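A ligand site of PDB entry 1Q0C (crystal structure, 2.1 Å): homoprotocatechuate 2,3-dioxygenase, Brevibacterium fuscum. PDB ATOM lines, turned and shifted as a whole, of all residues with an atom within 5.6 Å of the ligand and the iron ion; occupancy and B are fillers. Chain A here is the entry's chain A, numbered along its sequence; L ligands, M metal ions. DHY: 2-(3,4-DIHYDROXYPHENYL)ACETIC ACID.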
ATOM      1  N   HIS A 155       9.072 -35.378  -9.326  1.00  0.00           N
ATOM      2  CA  HIS A 155       7.771 -34.692  -9.486  1.00  0.00           C
ATOM      3  C   HIS A 155       7.516 -34.140 -10.867  1.00  0.00           C
ATOM      4  O   HIS A 155       8.392 -34.129 -11.750  1.00  0.00           O
ATOM      5  CB  HIS A 155       7.681 -33.477  -8.525  1.00  0.00           C
ATOM      6  CG  HIS A 155       8.671 -32.366  -8.838  1.00  0.00           C
ATOM      7  ND1 HIS A 155       9.847 -32.190  -8.132  1.00  0.00           N
ATOM      8  CD2 HIS A 155       8.640 -31.378  -9.770  1.00  0.00           C
ATOM      9  CE1 HIS A 155      10.492 -31.123  -8.606  1.00  0.00           C
ATOM     10  NE2 HIS A 155       9.783 -30.621  -9.608  1.00  0.00           N
ATOM     11  N   ASN A 157       5.285 -30.716 -12.804  1.00  0.00           N
ATOM     12  CA  ASN A 157       4.863 -29.339 -12.581  1.00  0.00           C
ATOM     13  C   ASN A 157       3.969 -28.961 -13.790  1.00  0.00           C
ATOM     14  O   ASN A 157       4.457 -28.910 -14.941  1.00  0.00           O
ATOM     15  CB  ASN A 157       6.049 -28.407 -12.519  1.00  0.00           C
ATOM     16  CG  ASN A 157       5.657 -27.038 -12.101  1.00  0.00           C
ATOM     17  OD1 ASN A 157       4.738 -26.499 -12.669  1.00  0.00           O
ATOM     18  ND2 ASN A 157       6.343 -26.457 -11.115  1.00  0.00           N
ATOM     19  N   TRP A 192       2.488 -26.176  -4.413  1.00  0.00           N
ATOM     20  CA  TRP A 192       3.299 -27.394  -4.482  1.00  0.00           C
ATOM     21  C   TRP A 192       2.615 -28.402  -3.619  1.00  0.00           C
ATOM     22  O   TRP A 192       2.261 -28.082  -2.486  1.00  0.00           O
ATOM     23  CB  TRP A 192       4.723 -27.101  -3.991  1.00  0.00           C
ATOM     24  CG  TRP A 192       5.546 -26.334  -5.001  1.00  0.00           C
ATOM     25  CD1 TRP A 192       6.523 -26.848  -5.774  1.00  0.00           C
ATOM     26  CD2 TRP A 192       5.464 -24.938  -5.328  1.00  0.00           C
ATOM     27  NE1 TRP A 192       7.081 -25.868  -6.558  1.00  0.00           N
ATOM     28  CE2 TRP A 192       6.452 -24.674  -6.310  1.00  0.00           C
ATOM     29  CE3 TRP A 192       4.668 -23.875  -4.879  1.00  0.00           C
ATOM     30  CZ2 TRP A 192       6.669 -23.388  -6.858  1.00  0.00           C
ATOM     31  CZ3 TRP A 192       4.867 -22.609  -5.407  1.00  0.00           C
ATOM     32  CH2 TRP A 192       5.878 -22.369  -6.400  1.00  0.00           C
ATOM     33  N   HIS A 200       6.976 -32.066  -3.102  1.00  0.00           N
ATOM     34  CA  HIS A 200       5.855 -32.305  -4.041  1.00  0.00           C
ATOM     35  C   HIS A 200       5.944 -33.498  -4.973  1.00  0.00           C
ATOM     36  O   HIS A 200       7.027 -34.065  -5.178  1.00  0.00           O
ATOM     37  CB  HIS A 200       5.561 -31.084  -4.911  1.00  0.00           C
ATOM     38  CG  HIS A 200       6.737 -30.604  -5.711  1.00  0.00           C
ATOM     39  ND1 HIS A 200       8.015 -30.551  -5.204  1.00  0.00           N
ATOM     40  CD2 HIS A 200       6.797 -30.032  -6.941  1.00  0.00           C
ATOM     41  CE1 HIS A 200       8.802 -29.952  -6.073  1.00  0.00           C
ATOM     42  NE2 HIS A 200       8.091 -29.621  -7.131  1.00  0.00           N
ATOM     43  N   HIS A 214       7.328 -29.135 -16.572  1.00  0.00           N
ATOM     44  CA  HIS A 214       8.521 -29.995 -16.541  1.00  0.00           C
ATOM     45  C   HIS A 214       8.351 -31.282 -15.749  1.00  0.00           C
ATOM     46  O   HIS A 214       7.376 -31.483 -15.022  1.00  0.00           O
ATOM     47  CB  HIS A 214       9.757 -29.210 -16.025  1.00  0.00           C
ATOM     48  CG  HIS A 214       9.633 -28.701 -14.616  1.00  0.00           C
ATOM     49  ND1 HIS A 214       9.166 -27.431 -14.326  1.00  0.00           N
ATOM     50  CD2 HIS A 214       9.781 -29.330 -13.434  1.00  0.00           C
ATOM     51  CE1 HIS A 214       9.022 -27.318 -13.017  1.00  0.00           C
ATOM     52  NE2 HIS A 214       9.386 -28.454 -12.461  1.00  0.00           N
ATOM     53  N   ALA A 216      10.748 -33.666 -13.178  1.00  0.00           N
ATOM     54  CA  ALA A 216      11.990 -33.502 -12.408  1.00  0.00           C
ATOM     55  C   ALA A 216      12.593 -34.780 -11.905  1.00  0.00           C
ATOM     56  O   ALA A 216      11.884 -35.663 -11.403  1.00  0.00           O
ATOM     57  CB  ALA A 216      11.758 -32.601 -11.199  1.00  0.00           C
ATOM     58  N   ARG A 243      17.701 -22.649 -17.278  1.00  0.00           N
ATOM     59  CA  ARG A 243      17.744 -21.839 -16.081  1.00  0.00           C
ATOM     60  C   ARG A 243      18.529 -22.592 -14.992  1.00  0.00           C
ATOM     61  O   ARG A 243      18.350 -23.785 -14.797  1.00  0.00           O
ATOM     62  CB  ARG A 243      16.281 -21.577 -15.619  1.00  0.00           C
ATOM     63  CG  ARG A 243      16.136 -20.902 -14.300  1.00  0.00           C
ATOM     64  CD  ARG A 243      14.708 -20.682 -13.913  1.00  0.00           C
ATOM     65  NE  ARG A 243      14.686 -20.141 -12.563  1.00  0.00           N
ATOM     66  CZ  ARG A 243      13.740 -20.402 -11.671  1.00  0.00           C
ATOM     67  NH1 ARG A 243      12.724 -21.202 -11.985  1.00  0.00           N
ATOM     68  NH2 ARG A 243      13.841 -19.895 -10.441  1.00  0.00           N
ATOM     69  N   HIS A 248      16.499 -23.027  -5.093  1.00  0.00           N
ATOM     70  CA  HIS A 248      15.119 -22.515  -5.128  1.00  0.00           C
ATOM     71  C   HIS A 248      14.773 -21.928  -3.755  1.00  0.00           C
ATOM     72  O   HIS A 248      15.265 -22.425  -2.714  1.00  0.00           O
ATOM     73  CB  HIS A 248      14.102 -23.659  -5.302  1.00  0.00           C
ATOM     74  CG  HIS A 248      13.935 -24.157  -6.701  1.00  0.00           C
ATOM     75  ND1 HIS A 248      13.714 -23.316  -7.781  1.00  0.00           N
ATOM     76  CD2 HIS A 248      13.864 -25.431  -7.189  1.00  0.00           C
ATOM     77  CE1 HIS A 248      13.511 -24.055  -8.875  1.00  0.00           C
ATOM     78  NE2 HIS A 248      13.602 -25.332  -8.542  1.00  0.00           N
ATOM     79  N   GLY A 249      13.928 -20.882  -3.726  1.00  0.00           N
ATOM     80  CA  GLY A 249      13.435 -20.367  -2.452  1.00  0.00           C
ATOM     81  C   GLY A 249      12.383 -21.409  -2.083  1.00  0.00           C
ATOM     82  O   GLY A 249      12.564 -22.183  -1.153  1.00  0.00           O
ATOM     83  N   VAL A 250      11.282 -21.448  -2.823  1.00  0.00           N
ATOM     84  CA  VAL A 250      10.255 -22.472  -2.601  1.00  0.00           C
ATOM     85  C   VAL A 250      10.943 -23.848  -2.752  1.00  0.00           C
ATOM     86  O   VAL A 250      11.665 -24.066  -3.734  1.00  0.00           O
ATOM     87  CB  VAL A 250       9.102 -22.395  -3.677  1.00  0.00           C
ATOM     88  CG1 VAL A 250       8.065 -23.491  -3.418  1.00  0.00           C
ATOM     89  CG2 VAL A 250       8.398 -21.074  -3.618  1.00  0.00           C
ATOM     90  N   SER A 251      10.705 -24.743  -1.792  1.00  0.00           N
ATOM     91  CA  SER A 251      11.272 -26.111  -1.772  1.00  0.00           C
ATOM     92  C   SER A 251      12.684 -26.194  -1.226  1.00  0.00           C
ATOM     93  O   SER A 251      13.078 -27.261  -0.758  1.00  0.00           O
ATOM     94  CB  SER A 251      11.264 -26.786  -3.148  1.00  0.00           C
ATOM     95  OG  SER A 251      12.424 -26.461  -3.890  1.00  0.00           O
ATOM     96  N   TYR A 255      18.813 -26.659  -7.965  1.00  0.00           N
ATOM     97  CA  TYR A 255      18.144 -27.075  -9.222  1.00  0.00           C
ATOM     98  C   TYR A 255      18.835 -26.659 -10.495  1.00  0.00           C
ATOM     99  O   TYR A 255      19.746 -25.861 -10.477  1.00  0.00           O
ATOM    100  CB  TYR A 255      16.729 -26.448  -9.228  1.00  0.00           C
ATOM    101  CG  TYR A 255      16.777 -24.940  -9.500  1.00  0.00           C
ATOM    102  CD1 TYR A 255      16.843 -24.452 -10.819  1.00  0.00           C
ATOM    103  CD2 TYR A 255      16.848 -24.015  -8.452  1.00  0.00           C
ATOM    104  CE1 TYR A 255      16.981 -23.054 -11.095  1.00  0.00           C
ATOM    105  CE2 TYR A 255      16.983 -22.605  -8.710  1.00  0.00           C
ATOM    106  CZ  TYR A 255      17.039 -22.152 -10.033  1.00  0.00           C
ATOM    107  OH  TYR A 255      17.116 -20.824 -10.322  1.00  0.00           O
ATOM    108  N   TYR A 257      17.489 -26.542 -14.925  1.00  0.00           N
ATOM    109  CA  TYR A 257      16.457 -26.775 -15.947  1.00  0.00           C
ATOM    110  C   TYR A 257      17.118 -26.845 -17.273  1.00  0.00           C
ATOM    111  O   TYR A 257      17.858 -25.936 -17.660  1.00  0.00           O
ATOM    112  CB  TYR A 257      15.415 -25.663 -16.035  1.00  0.00           C
ATOM    113  CG  TYR A 257      14.518 -25.617 -14.813  1.00  0.00           C
ATOM    114  CD1 TYR A 257      13.423 -26.468 -14.677  1.00  0.00           C
ATOM    115  CD2 TYR A 257      14.800 -24.713 -13.788  1.00  0.00           C
ATOM    116  CE1 TYR A 257      12.628 -26.437 -13.520  1.00  0.00           C
ATOM    117  CE2 TYR A 257      14.015 -24.672 -12.642  1.00  0.00           C
ATOM    118  CZ  TYR A 257      12.929 -25.513 -12.517  1.00  0.00           C
ATOM    119  OH  TYR A 257      12.155 -25.365 -11.384  1.00  0.00           O
ATOM    120  N   GLU A 267      13.806 -31.018 -15.172  1.00  0.00           N
ATOM    121  CA  GLU A 267      14.487 -30.328 -14.082  1.00  0.00           C
ATOM    122  C   GLU A 267      15.315 -31.353 -13.323  1.00  0.00           C
ATOM    123  O   GLU A 267      14.868 -32.504 -13.181  1.00  0.00           O
ATOM    124  CB  GLU A 267      13.512 -29.680 -13.092  1.00  0.00           C
ATOM    125  CG  GLU A 267      14.246 -28.988 -11.965  1.00  0.00           C
ATOM    126  CD  GLU A 267      13.310 -28.563 -10.848  1.00  0.00           C
ATOM    127  OE1 GLU A 267      12.188 -29.115 -10.787  1.00  0.00           O
ATOM    128  OE2 GLU A 267      13.699 -27.702 -10.029  1.00  0.00           O
ATOM    129  N   TYR A 269      17.142 -31.768  -9.685  1.00  0.00           N
ATOM    130  CA  TYR A 269      16.892 -31.213  -8.361  1.00  0.00           C
ATOM    131  C   TYR A 269      17.525 -32.057  -7.274  1.00  0.00           C
ATOM    132  O   TYR A 269      17.627 -33.276  -7.441  1.00  0.00           O
ATOM    133  CB  TYR A 269      15.370 -31.340  -8.277  1.00  0.00           C
ATOM    134  CG  TYR A 269      14.586 -31.018  -7.059  1.00  0.00           C
ATOM    135  CD1 TYR A 269      14.423 -31.950  -6.003  1.00  0.00           C
ATOM    136  CD2 TYR A 269      13.762 -29.862  -7.076  1.00  0.00           C
ATOM    137  CE1 TYR A 269      13.400 -31.716  -5.033  1.00  0.00           C
ATOM    138  CE2 TYR A 269      12.780 -29.622  -6.159  1.00  0.00           C
ATOM    139  CZ  TYR A 269      12.583 -30.530  -5.137  1.00  0.00           C
ATOM    140  OH  TYR A 269      11.508 -30.274  -4.331  1.00  0.00           O
ATOM    141  N   ARG A 292      11.676 -15.852  -3.612  1.00  0.00           N
ATOM    142  CA  ARG A 292      10.813 -17.026  -3.663  1.00  0.00           C
ATOM    143  C   ARG A 292      11.162 -18.065  -4.741  1.00  0.00           C
ATOM    144  O   ARG A 292      10.954 -19.256  -4.542  1.00  0.00           O
ATOM    145  CB  ARG A 292       9.334 -16.620  -3.852  1.00  0.00           C
ATOM    146  CG  ARG A 292       9.035 -15.905  -5.140  1.00  0.00           C
ATOM    147  CD  ARG A 292       7.545 -15.421  -5.175  1.00  0.00           C
ATOM    148  NE  ARG A 292       7.156 -15.090  -6.539  1.00  0.00           N
ATOM    149  CZ  ARG A 292       7.654 -14.073  -7.239  1.00  0.00           C
ATOM    150  NH1 ARG A 292       8.578 -13.259  -6.696  1.00  0.00           N
ATOM    151  NH2 ARG A 292       7.302 -13.913  -8.513  1.00  0.00           N
ATOM    152  N   ARG A 293      11.681 -17.642  -5.879  1.00  0.00           N
ATOM    153  CA  ARG A 293      11.958 -18.653  -6.929  1.00  0.00           C
ATOM    154  C   ARG A 293      13.420 -18.995  -6.872  1.00  0.00           C
ATOM    155  O   ARG A 293      13.780 -20.157  -6.620  1.00  0.00           O
ATOM    156  CB  ARG A 293      11.580 -18.138  -8.328  1.00  0.00           C
ATOM    157  CG  ARG A 293      10.253 -17.386  -8.340  1.00  0.00           C
ATOM    158  CD  ARG A 293       9.293 -17.690  -9.514  1.00  0.00           C
ATOM    159  NE  ARG A 293       8.699 -19.010  -9.401  1.00  0.00           N
ATOM    160  CZ  ARG A 293       7.535 -19.348  -9.922  1.00  0.00           C
ATOM    161  NH1 ARG A 293       6.825 -18.442 -10.595  1.00  0.00           N
ATOM    162  NH2 ARG A 293       7.092 -20.601  -9.822  1.00  0.00           N
ATOM    163  N   ASP A 294      14.258 -18.004  -7.083  1.00  0.00           N
ATOM    164  CA  ASP A 294      15.666 -18.251  -6.977  1.00  0.00           C
ATOM    165  C   ASP A 294      16.126 -17.504  -5.729  1.00  0.00           C
ATOM    166  O   ASP A 294      16.131 -16.243  -5.661  1.00  0.00           O
ATOM    167  CB  ASP A 294      16.382 -17.786  -8.241  1.00  0.00           C
ATOM    168  CG  ASP A 294      17.855 -18.089  -8.194  1.00  0.00           C
ATOM    169  OD1 ASP A 294      18.599 -17.267  -7.613  1.00  0.00           O
ATOM    170  OD2 ASP A 294      18.260 -19.167  -8.705  1.00  0.00           O
ATOM    171  N   VAL A 300      14.869 -14.542 -13.438  1.00  0.00           N
ATOM    172  CA  VAL A 300      14.191 -15.745 -13.985  1.00  0.00           C
ATOM    173  C   VAL A 300      14.022 -15.648 -15.519  1.00  0.00           C
ATOM    174  O   VAL A 300      13.295 -14.795 -16.025  1.00  0.00           O
ATOM    175  CB  VAL A 300      12.745 -15.936 -13.375  1.00  0.00           C
ATOM    176  CG1 VAL A 300      12.172 -17.280 -13.785  1.00  0.00           C
ATOM    177  CG2 VAL A 300      12.763 -15.850 -11.860  1.00  0.00           C
ATOM    178  N   TRP A 304      11.210 -19.478 -19.404  1.00  0.00           N
ATOM    179  CA  TRP A 304      10.823 -20.344 -18.314  1.00  0.00           C
ATOM    180  C   TRP A 304       9.348 -20.109 -17.980  1.00  0.00           C
ATOM    181  O   TRP A 304       8.661 -21.005 -17.508  1.00  0.00           O
ATOM    182  CB  TRP A 304      11.723 -20.112 -17.072  1.00  0.00           C
ATOM    183  CG  TRP A 304      11.655 -21.224 -16.025  1.00  0.00           C
ATOM    184  CD1 TRP A 304      12.384 -22.397 -16.002  1.00  0.00           C
ATOM    185  CD2 TRP A 304      10.748 -21.305 -14.937  1.00  0.00           C
ATOM    186  NE1 TRP A 304      11.975 -23.205 -14.981  1.00  0.00           N
ATOM    187  CE2 TRP A 304      10.967 -22.561 -14.300  1.00  0.00           C
ATOM    188  CE3 TRP A 304       9.757 -20.458 -14.426  1.00  0.00           C
ATOM    189  CZ2 TRP A 304      10.231 -22.976 -13.203  1.00  0.00           C
ATOM    190  CZ3 TRP A 304       9.031 -20.858 -13.316  1.00  0.00           C
ATOM    191  CH2 TRP A 304       9.271 -22.107 -12.719  1.00  0.00           C
ATOM    192  N   TYR A 305       8.852 -18.893 -18.234  1.00  0.00           N
ATOM    193  CA  TYR A 305       7.450 -18.592 -17.917  1.00  0.00           C
ATOM    194  C   TYR A 305       6.510 -18.804 -19.091  1.00  0.00           C
ATOM    195  O   TYR A 305       5.332 -19.102 -18.921  1.00  0.00           O
ATOM    196  CB  TYR A 305       7.305 -17.143 -17.438  1.00  0.00           C
ATOM    197  CG  TYR A 305       7.820 -16.909 -16.053  1.00  0.00           C
ATOM    198  CD1 TYR A 305       7.199 -17.517 -14.958  1.00  0.00           C
ATOM    199  CD2 TYR A 305       8.886 -16.052 -15.820  1.00  0.00           C
ATOM    200  CE1 TYR A 305       7.627 -17.269 -13.654  1.00  0.00           C
ATOM    201  CE2 TYR A 305       9.329 -15.791 -14.512  1.00  0.00           C
ATOM    202  CZ  TYR A 305       8.683 -16.406 -13.444  1.00  0.00           C
ATOM    203  OH  TYR A 305       9.101 -16.174 -12.154  1.00  0.00           O
HETATM  204  C1  DHY L   1      10.108 -23.586  -7.941  1.00  0.00           C
HETATM  205  C2  DHY L   1       9.881 -24.325  -9.156  1.00  0.00           C
HETATM  206  C3  DHY L   1      10.032 -25.733  -9.179  1.00  0.00           C
HETATM  207  C4  DHY L   1      10.400 -26.430  -7.980  1.00  0.00           C
HETATM  208  C5  DHY L   1      10.615 -25.710  -6.764  1.00  0.00           C
HETATM  209  C6  DHY L   1      10.471 -24.284  -6.758  1.00  0.00           C
HETATM  210  C7  DHY L   1       9.951 -22.120  -8.065  1.00  0.00           C
HETATM  211  C8  DHY L   1      11.000 -21.484  -8.934  1.00  0.00           C
HETATM  212  O1  DHY L   1      10.659 -20.946 -10.004  1.00  0.00           O
HETATM  213  O2  DHY L   1      12.238 -21.441  -8.739  1.00  0.00           O
HETATM  214  O3  DHY L   1       9.872 -26.632 -10.224  1.00  0.00           O
HETATM  215  O4  DHY L   1      10.495 -27.816  -8.197  1.00  0.00           O
HETATM  216 FE    FE M   1      10.232 -28.557 -10.351  1.00  0.00          FE
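The backbone carbonyl oxygen of Arg 293 lies close to a ring nitrogen (ND1) of His 248.
The backbone carbonyl oxygen of Arg 293 sits at hydrogen-bond distance from the backbone NH of Gly 249 (3.0 Å).
N of Asn 157 lies within hydrogen-bond range of O of His 214, 3.1 Å away.
ND1 of His 155 lies close to NE2 of His 200, 3.3 Å away.
OH of Tyr 257 is in hydrogen-bond range of OE2 of Glu 267, 3.1 Å away.
O of His 155 is in hydrogen-bond range of N of Ala 216, 2.8 Å away.
The backbone carbonyl oxygen (O) of Arg 243 lies within hydrogen-bond range of the backbone NH (N) of Tyr 257 (2.9 Å).
The guanidinium group of Arg 243 is in hydrogen-bond range of the side-chain hydroxyl of Tyr 255.
Asn 157 touches the ligand (ND2 to O3, 3.6 Å).
Trp 192 touches the ligand (NE1 to C5, 3.5 Å).
Val 250 touches the ligand.
Ser 251 touches the ligand.
Tyr 269 touches the ligand (CE2 to O4, 3.6 Å).
Trp 304 touches the ligand.
Hydrophobic or aromatic side chains that line the ligand: His 155, Trp 192, His 200, His 214, His 248, Val 250, Tyr 257, Tyr 269 and Trp 304.
Along chain A the residues within 4 Å of the ligand span positions 155 to 304.
The iron ion is bound by O3 of the ligand, OE1 of Glu 267, NE2 of His 155, NE2 of His 214 and O4 of the ligand.
The iron ion has five donor atoms within binding distance.
OH of Tyr 257 touches the iron ion (3.9 Å).
Four residues have an atom within 4 Å of the iron ion: His 155, His 214, Tyr 257 and Glu 267.
The guanidinium group (NH2) of Arg 243 lies within salt-bridge range of an oxygen (O2) of the ligand (2.8 Å).
NE of Arg 293 lies within salt-bridge range of O1 of the ligand, at 2.8 Å.
O3 of the ligand sits close to OH of Tyr 257 (2.9 Å).
A ring nitrogen (NE2) of His 200 sits close to an oxygen (O4) of the ligand (3.2 Å).
ND1 of His 248 sits at hydrogen-bond distance from O2 of the ligand (2.6 Å).
O of Arg 293 sits close to O2 of the ligand (2.9 Å).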
